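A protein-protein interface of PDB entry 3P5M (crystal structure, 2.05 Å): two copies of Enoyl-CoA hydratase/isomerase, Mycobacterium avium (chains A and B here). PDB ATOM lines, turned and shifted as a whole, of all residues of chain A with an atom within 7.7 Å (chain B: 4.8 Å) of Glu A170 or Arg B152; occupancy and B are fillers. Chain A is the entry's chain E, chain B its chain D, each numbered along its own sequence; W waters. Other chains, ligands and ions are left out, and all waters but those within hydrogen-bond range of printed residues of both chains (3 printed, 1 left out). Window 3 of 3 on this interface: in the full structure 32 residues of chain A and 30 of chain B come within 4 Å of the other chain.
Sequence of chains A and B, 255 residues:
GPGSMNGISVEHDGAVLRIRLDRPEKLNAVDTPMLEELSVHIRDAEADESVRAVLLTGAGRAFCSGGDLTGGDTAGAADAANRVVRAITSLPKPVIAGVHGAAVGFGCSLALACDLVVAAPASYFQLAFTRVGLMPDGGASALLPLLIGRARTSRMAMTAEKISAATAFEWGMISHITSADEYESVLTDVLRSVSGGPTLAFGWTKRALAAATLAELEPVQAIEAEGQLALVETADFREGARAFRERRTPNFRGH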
ATOM      1  N   ASP A 115       8.315 -10.844   4.421  1.00  0.00           N
ATOM      2  CA  ASP A 115       8.002 -11.071   3.030  1.00  0.00           C
ATOM      3  C   ASP A 115       9.129 -10.755   2.061  1.00  0.00           C
ATOM      4  O   ASP A 115       9.346 -11.521   1.102  1.00  0.00           O
ATOM      5  CB  ASP A 115       6.734 -10.332   2.692  1.00  0.00           C
ATOM      6  CG  ASP A 115       5.626 -10.735   3.613  1.00  0.00           C
ATOM      7  OD1 ASP A 115       5.248 -11.926   3.572  1.00  0.00           O
ATOM      8  OD2 ASP A 115       5.188  -9.891   4.426  1.00  0.00           O
ATOM      9  N   LEU A 116       9.830  -9.635   2.289  1.00  0.00           N
ATOM     10  CA  LEU A 116      10.998  -9.254   1.489  1.00  0.00           C
ATOM     11  C   LEU A 116      12.110  -8.865   2.449  1.00  0.00           C
ATOM     12  O   LEU A 116      11.858  -8.380   3.551  1.00  0.00           O
ATOM     13  CB  LEU A 116      10.683  -8.056   0.562  1.00  0.00           C
ATOM     14  CG  LEU A 116       9.483  -8.218  -0.404  1.00  0.00           C
ATOM     15  CD1 LEU A 116       8.973  -6.859  -0.952  1.00  0.00           C
ATOM     16  CD2 LEU A 116       9.733  -9.263  -1.523  1.00  0.00           C
ATOM     17  N   LEU A 146      12.610 -24.090   3.058  1.00  0.00           N
ATOM     18  CA  LEU A 146      11.721 -23.661   1.952  1.00  0.00           C
ATOM     19  C   LEU A 146      12.271 -22.409   1.265  1.00  0.00           C
ATOM     20  O   LEU A 146      11.674 -21.874   0.329  1.00  0.00           O
ATOM     21  CB  LEU A 146      10.287 -23.424   2.447  1.00  0.00           C
ATOM     22  CG  LEU A 146       9.317 -24.617   2.462  1.00  0.00           C
ATOM     23  CD1 LEU A 146       9.081 -25.222   1.047  1.00  0.00           C
ATOM     24  CD2 LEU A 146       9.705 -25.726   3.476  1.00  0.00           C
ATOM     25  N   LEU A 147      13.429 -21.976   1.733  1.00  0.00           N
ATOM     26  CA  LEU A 147      14.185 -20.913   1.111  1.00  0.00           C
ATOM     27  C   LEU A 147      15.371 -21.461   0.359  1.00  0.00           C
ATOM     28  O   LEU A 147      15.501 -21.217  -0.848  1.00  0.00           O
ATOM     29  CB  LEU A 147      14.648 -19.869   2.163  1.00  0.00           C
ATOM     30  CG  LEU A 147      13.510 -19.152   2.902  1.00  0.00           C
ATOM     31  CD1 LEU A 147      14.062 -18.354   4.109  1.00  0.00           C
ATOM     32  CD2 LEU A 147      12.793 -18.227   1.912  1.00  0.00           C
ATOM     33  N   ILE A 148      16.234 -22.203   1.054  1.00  0.00           N
ATOM     34  CA  ILE A 148      17.499 -22.588   0.470  1.00  0.00           C
ATOM     35  C   ILE A 148      17.725 -24.086   0.379  1.00  0.00           C
ATOM     36  O   ILE A 148      18.817 -24.522  -0.005  1.00  0.00           O
ATOM     37  CB  ILE A 148      18.691 -21.978   1.306  1.00  0.00           C
ATOM     38  CG1 ILE A 148      18.746 -22.653   2.704  1.00  0.00           C
ATOM     39  CG2 ILE A 148      18.575 -20.504   1.341  1.00  0.00           C
ATOM     40  CD1 ILE A 148      19.950 -22.201   3.616  1.00  0.00           C
ATOM     41  N   ARG A 152      21.789 -26.958   2.464  1.00  0.00           N
ATOM     42  CA  ARG A 152      22.326 -25.686   2.906  1.00  0.00           C
ATOM     43  C   ARG A 152      21.841 -25.335   4.293  1.00  0.00           C
ATOM     44  O   ARG A 152      22.590 -24.715   5.054  1.00  0.00           O
ATOM     45  CB  ARG A 152      21.969 -24.557   1.912  1.00  0.00           C
ATOM     46  CG  ARG A 152      22.674 -24.717   0.578  1.00  0.00           C
ATOM     47  CD  ARG A 152      22.120 -23.789  -0.561  1.00  0.00           C
ATOM     48  NE  ARG A 152      23.171 -23.710  -1.561  1.00  0.00           N
ATOM     49  CZ  ARG A 152      23.047 -23.422  -2.840  1.00  0.00           C
ATOM     50  NH1 ARG A 152      24.159 -23.421  -3.587  1.00  0.00           N
ATOM     51  NH2 ARG A 152      21.866 -23.125  -3.360  1.00  0.00           N
ATOM     52  N   SER A 164      27.300 -14.620   3.701  1.00  0.00           N
ATOM     53  CA  SER A 164      27.267 -13.242   3.196  1.00  0.00           C
ATOM     54  C   SER A 164      25.909 -12.914   2.603  1.00  0.00           C
ATOM     55  O   SER A 164      25.155 -13.794   2.186  1.00  0.00           O
ATOM     56  CB  SER A 164      28.355 -13.024   2.139  1.00  0.00           C
ATOM     57  OG  SER A 164      28.106 -13.817   0.979  1.00  0.00           O
ATOM     58  N   ALA A 165      25.584 -11.633   2.549  1.00  0.00           N
ATOM     59  CA  ALA A 165      24.414 -11.227   1.810  1.00  0.00           C
ATOM     60  C   ALA A 165      24.409 -11.707   0.350  1.00  0.00           C
ATOM     61  O   ALA A 165      23.374 -12.169  -0.153  1.00  0.00           O
ATOM     62  CB  ALA A 165      24.244  -9.736   1.884  1.00  0.00           C
ATOM     63  N   ALA A 166      25.542 -11.583  -0.338  1.00  0.00           N
ATOM     64  CA  ALA A 166      25.651 -12.061  -1.724  1.00  0.00           C
ATOM     65  C   ALA A 166      25.288 -13.530  -1.823  1.00  0.00           C
ATOM     66  O   ALA A 166      24.434 -13.911  -2.631  1.00  0.00           O
ATOM     67  CB  ALA A 166      27.082 -11.800  -2.323  1.00  0.00           C
ATOM     68  N   THR A 167      25.911 -14.353  -0.986  1.00  0.00           N
ATOM     69  CA  THR A 167      25.591 -15.783  -0.973  1.00  0.00           C
ATOM     70  C   THR A 167      24.138 -16.079  -0.641  1.00  0.00           C
ATOM     71  O   THR A 167      23.478 -16.876  -1.342  1.00  0.00           O
ATOM     72  CB  THR A 167      26.526 -16.542  -0.047  1.00  0.00           C
ATOM     73  OG1 THR A 167      27.874 -16.282  -0.456  1.00  0.00           O
ATOM     74  CG2 THR A 167      26.259 -18.049  -0.123  1.00  0.00           C
ATOM     75  N   ALA A 168      23.622 -15.444   0.406  1.00  0.00           N
ATOM     76  CA  ALA A 168      22.218 -15.625   0.757  1.00  0.00           C
ATOM     77  C   ALA A 168      21.324 -15.318  -0.452  1.00  0.00           C
ATOM     78  O   ALA A 168      20.360 -16.055  -0.711  1.00  0.00           O
ATOM     79  CB  ALA A 168      21.835 -14.757   1.964  1.00  0.00           C
ATOM     80  N   PHE A 169      21.629 -14.234  -1.167  1.00  0.00           N
ATOM     81  CA  PHE A 169      20.849 -13.864  -2.352  1.00  0.00           C
ATOM     82  C   PHE A 169      20.952 -14.929  -3.454  1.00  0.00           C
ATOM     83  O   PHE A 169      19.919 -15.316  -4.002  1.00  0.00           O
ATOM     84  CB  PHE A 169      21.325 -12.531  -2.923  1.00  0.00           C
ATOM     85  CG  PHE A 169      20.571 -12.089  -4.161  1.00  0.00           C
ATOM     86  CD1 PHE A 169      19.307 -11.507  -4.048  1.00  0.00           C
ATOM     87  CD2 PHE A 169      21.144 -12.211  -5.421  1.00  0.00           C
ATOM     88  CE1 PHE A 169      18.609 -11.081  -5.179  1.00  0.00           C
ATOM     89  CE2 PHE A 169      20.445 -11.786  -6.592  1.00  0.00           C
ATOM     90  CZ  PHE A 169      19.177 -11.221  -6.456  1.00  0.00           C
ATOM     91  N   GLU A 170      22.184 -15.370  -3.764  1.00  0.00           N
ATOM     92  CA  GLU A 170      22.435 -16.474  -4.728  1.00  0.00           C
ATOM     93  C   GLU A 170      21.629 -17.728  -4.414  1.00  0.00           C
ATOM     94  O   GLU A 170      21.162 -18.439  -5.319  1.00  0.00           O
ATOM     95  CB  GLU A 170      23.920 -16.912  -4.741  1.00  0.00           C
ATOM     96  CG  GLU A 170      24.178 -18.107  -5.702  1.00  0.00           C
ATOM     97  CD  GLU A 170      25.365 -18.994  -5.319  1.00  0.00           C
ATOM     98  OE1 GLU A 170      26.356 -18.486  -4.742  1.00  0.00           O
ATOM     99  OE2 GLU A 170      25.296 -20.220  -5.614  1.00  0.00           O
ATOM    100  N   TRP A 171      21.504 -18.015  -3.136  1.00  0.00           N
ATOM    101  CA  TRP A 171      20.852 -19.227  -2.650  1.00  0.00           C
ATOM    102  C   TRP A 171      19.323 -19.156  -2.622  1.00  0.00           C
ATOM    103  O   TRP A 171      18.655 -20.172  -2.351  1.00  0.00           O
ATOM    104  CB  TRP A 171      21.315 -19.492  -1.221  1.00  0.00           C
ATOM    105  CG  TRP A 171      22.705 -20.056  -1.018  1.00  0.00           C
ATOM    106  CD1 TRP A 171      23.694 -20.219  -1.948  1.00  0.00           C
ATOM    107  CD2 TRP A 171      23.257 -20.493   0.239  1.00  0.00           C
ATOM    108  NE1 TRP A 171      24.809 -20.766  -1.349  1.00  0.00           N
ATOM    109  CE2 TRP A 171      24.575 -20.929  -0.011  1.00  0.00           C
ATOM    110  CE3 TRP A 171      22.756 -20.560   1.548  1.00  0.00           C
ATOM    111  CZ2 TRP A 171      25.423 -21.414   1.021  1.00  0.00           C
ATOM    112  CZ3 TRP A 171      23.585 -21.052   2.560  1.00  0.00           C
ATOM    113  CH2 TRP A 171      24.893 -21.483   2.287  1.00  0.00           C
ATOM    114  N   GLY A 172      18.779 -17.956  -2.821  1.00  0.00           N
ATOM    115  CA  GLY A 172      17.332 -17.698  -2.664  1.00  0.00           C
ATOM    116  C   GLY A 172      16.847 -17.480  -1.237  1.00  0.00           C
ATOM    117  O   GLY A 172      15.652 -17.614  -0.958  1.00  0.00           O
ATOM    118  N   MET A 173      17.764 -17.202  -0.318  1.00  0.00           N
ATOM    119  CA  MET A 173      17.410 -16.988   1.079  1.00  0.00           C
ATOM    120  C   MET A 173      16.640 -15.707   1.259  1.00  0.00           C
ATOM    121  O   MET A 173      15.777 -15.641   2.131  1.00  0.00           O
ATOM    122  CB  MET A 173      18.662 -16.923   1.980  1.00  0.00           C
ATOM    123  CG  MET A 173      18.383 -17.158   3.462  1.00  0.00           C
ATOM    124  SD  MET A 173      19.776 -16.675   4.550  1.00  0.00           S
ATOM    125  CE  MET A 173      20.966 -17.950   4.076  1.00  0.00           C
ATOM    126  N   ILE A 174      16.955 -14.701   0.438  1.00  0.00           N
ATOM    127  CA  ILE A 174      16.447 -13.362   0.623  1.00  0.00           C
ATOM    128  C   ILE A 174      16.070 -12.738  -0.746  1.00  0.00           C
ATOM    129  O   ILE A 174      16.719 -12.997  -1.761  1.00  0.00           O
ATOM    130  CB  ILE A 174      17.505 -12.433   1.315  1.00  0.00           C
ATOM    131  CG1 ILE A 174      18.831 -12.450   0.515  1.00  0.00           C
ATOM    132  CG2 ILE A 174      17.719 -12.848   2.774  1.00  0.00           C
ATOM    133  CD1 ILE A 174      19.897 -11.394   0.937  1.00  0.00           C
ATOM    134  N   SER A 175      15.042 -11.898  -0.745  1.00  0.00           N
ATOM    135  CA  SER A 175      14.478 -11.403  -2.004  1.00  0.00           C
ATOM    136  C   SER A 175      15.392 -10.410  -2.729  1.00  0.00           C
ATOM    137  O   SER A 175      15.476 -10.430  -3.982  1.00  0.00           O
ATOM    138  CB  SER A 175      13.131 -10.742  -1.734  1.00  0.00           C
ATOM    139  OG  SER A 175      13.275  -9.650  -0.847  1.00  0.00           O
ATOM    140  N   HIS A 176      16.060  -9.550  -1.956  1.00  0.00           N
ATOM    141  CA  HIS A 176      16.836  -8.430  -2.529  1.00  0.00           C
ATOM    142  C   HIS A 176      18.260  -8.294  -1.969  1.00  0.00           C
ATOM    143  O   HIS A 176      18.477  -8.405  -0.733  1.00  0.00           O
ATOM    144  CB  HIS A 176      16.126  -7.102  -2.286  1.00  0.00           C
ATOM    145  CG  HIS A 176      14.817  -6.936  -3.018  1.00  0.00           C
ATOM    146  ND1 HIS A 176      13.640  -7.485  -2.564  1.00  0.00           N
ATOM    147  CD2 HIS A 176      14.490  -6.185  -4.099  1.00  0.00           C
ATOM    148  CE1 HIS A 176      12.656  -7.129  -3.375  1.00  0.00           C
ATOM    149  NE2 HIS A 176      13.141  -6.309  -4.291  1.00  0.00           N
ATOM    150  N   ILE A 177      19.186  -7.962  -2.854  1.00  0.00           N
ATOM    151  CA  ILE A 177      20.572  -7.664  -2.499  1.00  0.00           C
ATOM    152  C   ILE A 177      20.905  -6.236  -2.952  1.00  0.00           C
ATOM    153  O   ILE A 177      20.371  -5.730  -3.956  1.00  0.00           O
ATOM    154  CB  ILE A 177      21.567  -8.728  -3.123  1.00  0.00           C
ATOM    155  CG1 ILE A 177      23.020  -8.434  -2.762  1.00  0.00           C
ATOM    156  CG2 ILE A 177      21.502  -8.792  -4.614  1.00  0.00           C
ATOM    157  CD1 ILE A 177      23.371  -8.848  -1.377  1.00  0.00           C
ATOM    158  N   LEU A 209       0.668 -18.154  -0.007  1.00  0.00           N
ATOM    159  CA  LEU A 209       2.056 -18.543   0.197  1.00  0.00           C
ATOM    160  C   LEU A 209       2.270 -19.232   1.568  1.00  0.00           C
ATOM    161  O   LEU A 209       2.932 -20.283   1.640  1.00  0.00           O
ATOM    162  CB  LEU A 209       2.992 -17.324   0.070  1.00  0.00           C
ATOM    163  CG  LEU A 209       3.168 -16.889  -1.383  1.00  0.00           C
ATOM    164  CD1 LEU A 209       4.039 -15.619  -1.530  1.00  0.00           C
ATOM    165  CD2 LEU A 209       3.753 -18.058  -2.204  1.00  0.00           C
ATOM    166  N   ILE B 148      11.562 -22.479  -6.572  1.00  0.00           N
ATOM    167  CA  ILE B 148      12.548 -21.409  -6.434  1.00  0.00           C
ATOM    168  C   ILE B 148      12.683 -20.913  -5.017  1.00  0.00           C
ATOM    169  O   ILE B 148      13.501 -20.006  -4.737  1.00  0.00           O
ATOM    170  CB  ILE B 148      12.203 -20.183  -7.350  1.00  0.00           C
ATOM    171  CG1 ILE B 148      10.854 -19.571  -6.975  1.00  0.00           C
ATOM    172  CG2 ILE B 148      12.201 -20.601  -8.814  1.00  0.00           C
ATOM    173  CD1 ILE B 148      10.523 -18.238  -7.760  1.00  0.00           C
ATOM    174  N   GLY B 149      11.858 -21.485  -4.132  1.00  0.00           N
ATOM    175  CA  GLY B 149      11.865 -21.120  -2.720  1.00  0.00           C
ATOM    176  C   GLY B 149      10.935 -19.955  -2.438  1.00  0.00           C
ATOM    177  O   GLY B 149      10.484 -19.270  -3.370  1.00  0.00           O
ATOM    178  N   ARG B 150      10.642 -19.738  -1.150  1.00  0.00           N
ATOM    179  CA  ARG B 150       9.611 -18.795  -0.736  1.00  0.00           C
ATOM    180  C   ARG B 150       9.977 -17.317  -0.974  1.00  0.00           C
ATOM    181  O   ARG B 150       9.104 -16.514  -1.273  1.00  0.00           O
ATOM    182  CB  ARG B 150       9.228 -19.028   0.719  1.00  0.00           C
ATOM    183  CG  ARG B 150       8.197 -18.035   1.343  1.00  0.00           C
ATOM    184  CD  ARG B 150       7.920 -18.361   2.847  1.00  0.00           C
ATOM    185  NE  ARG B 150       7.866 -17.132   3.650  1.00  0.00           N
ATOM    186  CZ  ARG B 150       8.802 -16.739   4.512  1.00  0.00           C
ATOM    187  NH1 ARG B 150       8.666 -15.580   5.153  1.00  0.00           N
ATOM    188  NH2 ARG B 150       9.866 -17.496   4.757  1.00  0.00           N
ATOM    189  N   ALA B 151      11.255 -16.967  -0.815  1.00  0.00           N
ATOM    190  CA  ALA B 151      11.650 -15.558  -0.939  1.00  0.00           C
ATOM    191  C   ALA B 151      11.582 -15.107  -2.384  1.00  0.00           C
ATOM    192  O   ALA B 151      11.067 -14.025  -2.636  1.00  0.00           O
ATOM    193  CB  ALA B 151      13.071 -15.290  -0.355  1.00  0.00           C
ATOM    194  N   ARG B 152      12.062 -15.934  -3.336  1.00  0.00           N
ATOM    195  CA  ARG B 152      11.973 -15.560  -4.747  1.00  0.00           C
ATOM    196  C   ARG B 152      10.517 -15.519  -5.231  1.00  0.00           C
ATOM    197  O   ARG B 152      10.155 -14.680  -6.100  1.00  0.00           O
ATOM    198  CB  ARG B 152      12.808 -16.501  -5.647  1.00  0.00           C
ATOM    199  CG  ARG B 152      14.296 -16.179  -5.586  1.00  0.00           C
ATOM    200  CD  ARG B 152      15.168 -17.338  -6.076  1.00  0.00           C
ATOM    201  NE  ARG B 152      16.506 -16.803  -6.295  1.00  0.00           N
ATOM    202  CZ  ARG B 152      17.652 -17.476  -6.320  1.00  0.00           C
ATOM    203  NH1 ARG B 152      18.802 -16.798  -6.509  1.00  0.00           N
ATOM    204  NH2 ARG B 152      17.672 -18.774  -6.151  1.00  0.00           N
ATOM    205  N   THR B 153       9.692 -16.431  -4.686  1.00  0.00           N
ATOM    206  CA  THR B 153       8.261 -16.423  -4.988  1.00  0.00           C
ATOM    207  C   THR B 153       7.583 -15.126  -4.453  1.00  0.00           C
ATOM    208  O   THR B 153       6.867 -14.449  -5.192  1.00  0.00           O
ATOM    209  CB  THR B 153       7.539 -17.676  -4.446  1.00  0.00           C
ATOM    210  OG1 THR B 153       8.157 -18.837  -4.979  1.00  0.00           O
ATOM    211  CG2 THR B 153       6.049 -17.660  -4.824  1.00  0.00           C
ATOM    212  N   SER B 154       7.814 -14.804  -3.174  1.00  0.00           N
ATOM    213  CA  SER B 154       7.247 -13.593  -2.605  1.00  0.00           C
ATOM    214  C   SER B 154       7.618 -12.404  -3.477  1.00  0.00           C
ATOM    215  O   SER B 154       6.746 -11.582  -3.818  1.00  0.00           O
ATOM    216  CB  SER B 154       7.734 -13.393  -1.177  1.00  0.00           C
ATOM    217  OG  SER B 154       7.119 -14.338  -0.327  1.00  0.00           O
ATOM    218  N   ARG B 155       8.907 -12.326  -3.854  1.00  0.00           N
ATOM    219  CA  ARG B 155       9.370 -11.291  -4.751  1.00  0.00           C
ATOM    220  C   ARG B 155       8.600 -11.255  -6.083  1.00  0.00           C
ATOM    221  O   ARG B 155       8.124 -10.193  -6.489  1.00  0.00           O
ATOM    222  CB  ARG B 155      10.886 -11.372  -5.040  1.00  0.00           C
ATOM    223  CG  ARG B 155      11.387 -10.023  -5.709  1.00  0.00           C
ATOM    224  CD  ARG B 155      12.915  -9.886  -5.821  1.00  0.00           C
ATOM    225  NE  ARG B 155      13.224  -8.880  -6.823  1.00  0.00           N
ATOM    226  CZ  ARG B 155      14.405  -8.281  -6.991  1.00  0.00           C
ATOM    227  NH1 ARG B 155      15.435  -8.563  -6.196  1.00  0.00           N
ATOM    228  NH2 ARG B 155      14.542  -7.360  -7.945  1.00  0.00           N
ATOM    229  N   MET B 156       8.487 -12.387  -6.770  1.00  0.00           N
ATOM    230  CA  MET B 156       7.796 -12.388  -8.064  1.00  0.00           C
ATOM    231  C   MET B 156       6.378 -11.900  -7.920  1.00  0.00           C
ATOM    232  O   MET B 156       5.877 -11.184  -8.762  1.00  0.00           O
ATOM    233  CB  MET B 156       7.777 -13.797  -8.677  1.00  0.00           C
ATOM    234  CG  MET B 156       9.109 -14.237  -9.257  1.00  0.00           C
ATOM    235  SD  MET B 156       8.962 -15.951  -9.885  1.00  0.00           S
ATOM    236  CE  MET B 156       7.991 -15.648 -11.402  1.00  0.00           C
ATOM    237  N   TRP B 171      17.655 -20.184 -11.100  1.00  0.00           N
ATOM    238  CA  TRP B 171      16.861 -20.412  -9.889  1.00  0.00           C
ATOM    239  C   TRP B 171      16.263 -21.840  -9.720  1.00  0.00           C
ATOM    240  O   TRP B 171      15.740 -22.142  -8.650  1.00  0.00           O
ATOM    241  CB  TRP B 171      15.659 -19.456  -9.908  1.00  0.00           C
ATOM    242  CG  TRP B 171      15.951 -18.014  -9.668  1.00  0.00           C
ATOM    243  CD1 TRP B 171      17.168 -17.435  -9.483  1.00  0.00           C
ATOM    244  CD2 TRP B 171      14.990 -16.963  -9.572  1.00  0.00           C
ATOM    245  NE1 TRP B 171      17.030 -16.080  -9.274  1.00  0.00           N
ATOM    246  CE2 TRP B 171      15.701 -15.764  -9.317  1.00  0.00           C
ATOM    247  CE3 TRP B 171      13.594 -16.909  -9.697  1.00  0.00           C
ATOM    248  CZ2 TRP B 171      15.064 -14.532  -9.177  1.00  0.00           C
ATOM    249  CZ3 TRP B 171      12.960 -15.682  -9.533  1.00  0.00           C
ATOM    250  CH2 TRP B 171      13.693 -14.516  -9.296  1.00  0.00           C
HETATM  251  O   HOH W   1       5.144 -13.720   1.616  1.00  0.00           O
HETATM  252  O   HOH W   2      17.320 -14.632  -3.881  1.00  0.00           O
HETATM  253  O   HOH W   3      17.894  -7.505  -5.687  1.00  0.00           O
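O of Leu A146 lies within hydrogen-bond range of N of Arg B150. NH1 of Arg B152 is in hydrogen-bond range of O of Phe A169 (3.1 Å). The guanidinium group of Arg B155 lies within hydrogen-bond range of the backbone carbonyl oxygen of Ser A175 (2.9 Å). The guanidinium group (NH1) of Arg B152 lies within hydrogen-bond range of the backbone carbonyl oxygen (O) of Glu A170 (3.1 Å).
The side-chain carboxylate of Glu A170 lies within salt-bridge range of the guanidinium group of Arg A152 (3.96 Å). OG of Ser A175 sits at hydrogen-bond distance from ND1 of His A176, at 2.8 Å. The backbone NH (N) of Met A173 sits at hydrogen-bond distance from the backbone carbonyl oxygen (O) of Ala A168, 2.9 Å away. OG1 of Thr B153 is in hydrogen-bond range of O of Gly B149, at 2.9 Å. The side-chain hydroxyl of Ser B154 sits at hydrogen-bond distance from the backbone carbonyl oxygen of Arg B150, at 3.1 Å.
Among the printed residues, merely in contact across the chains: Asp A115 with Ser B154, Leu A116 with Arg B155, Leu A146 with Gly B149, Leu A147 with Arg B150, Leu A147 with Ala B151, Trp A171 with Arg B152, Gly A172 with Ala B151, Gly A172 with Arg B152, Met A173 with Ala B151, Ile A174 with Ala B151, Ser A175 with Ala B151, His A176 with Arg B155, Leu A209 with Thr B153 and Leu A209 with Ser B154.
Of the printed residues of chain B, Glu A170 touches Arg B152. Of the printed residues of chain A, Arg B152 touches Phe A169 (3.1 Å), Glu A170 (3.1 Å), Trp A171 (3.9 Å) and Gly A172 (3.6 Å). Ala B151 touches five residues of chain A. Printed residues of chain B within 4 Å of Leu A116: Arg B155 (3.8 Å). Of the printed residues of chain B, Leu A209 touches Thr B153 (3.5 Å) and Ser B154 (3.5 Å). Printed residues of chain B within 4 Å of His A176: Arg B155 (3.3 Å). Of the printed residues of chain B, Met A173 touches Ala B151. Printed residues of chain B within 4 Å of Leu A146: Gly B149 and Arg B150. Ala A166 touches none of the printed residues of chain B. Trp B171 touches none of the printed residues of chain A. The nearest printed residue of chain B that does not touch Glu A170 is Trp B171 (5.9 Å). The nearest printed residue of chain A that does not touch Thr B153 is Asp A115 (6.9 Å).
Of the 10 printed residues of chain B, 7 touch a printed residue of chain A. Printed residues of chain B that touch a printed residue of chain A: Gly B149, Arg B150, Ala B151, Arg B152, Thr B153, Ser B154 and Arg B155. Hydrophobic or aromatic side chains of chain B that line the printed part of chain A: Ala B151. Among the printed residues, 18 pairs touch across the chains.
Trp A171 touches Arg B152, but with the chains exchanged Arg A152 does not touch Trp B171 (8.2 Å).
Water W1 bridges OD1 of Asp A115 (2.7 Å) and OG of Ser B154 (2.8 Å). Water W2 lies within hydrogen-bond range of the backbone carbonyl oxygen of Phe A169 (2.7 Å), the backbone carbonyl oxygen of Ile A174 (2.7 Å) and the guanidinium group of Arg B152 (3.3 Å). Water W3 bridges the guanidinium group (NH1) of Arg B155 (2.7 Å) and the backbone NH (N) of Ile A177 (3.1 Å).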
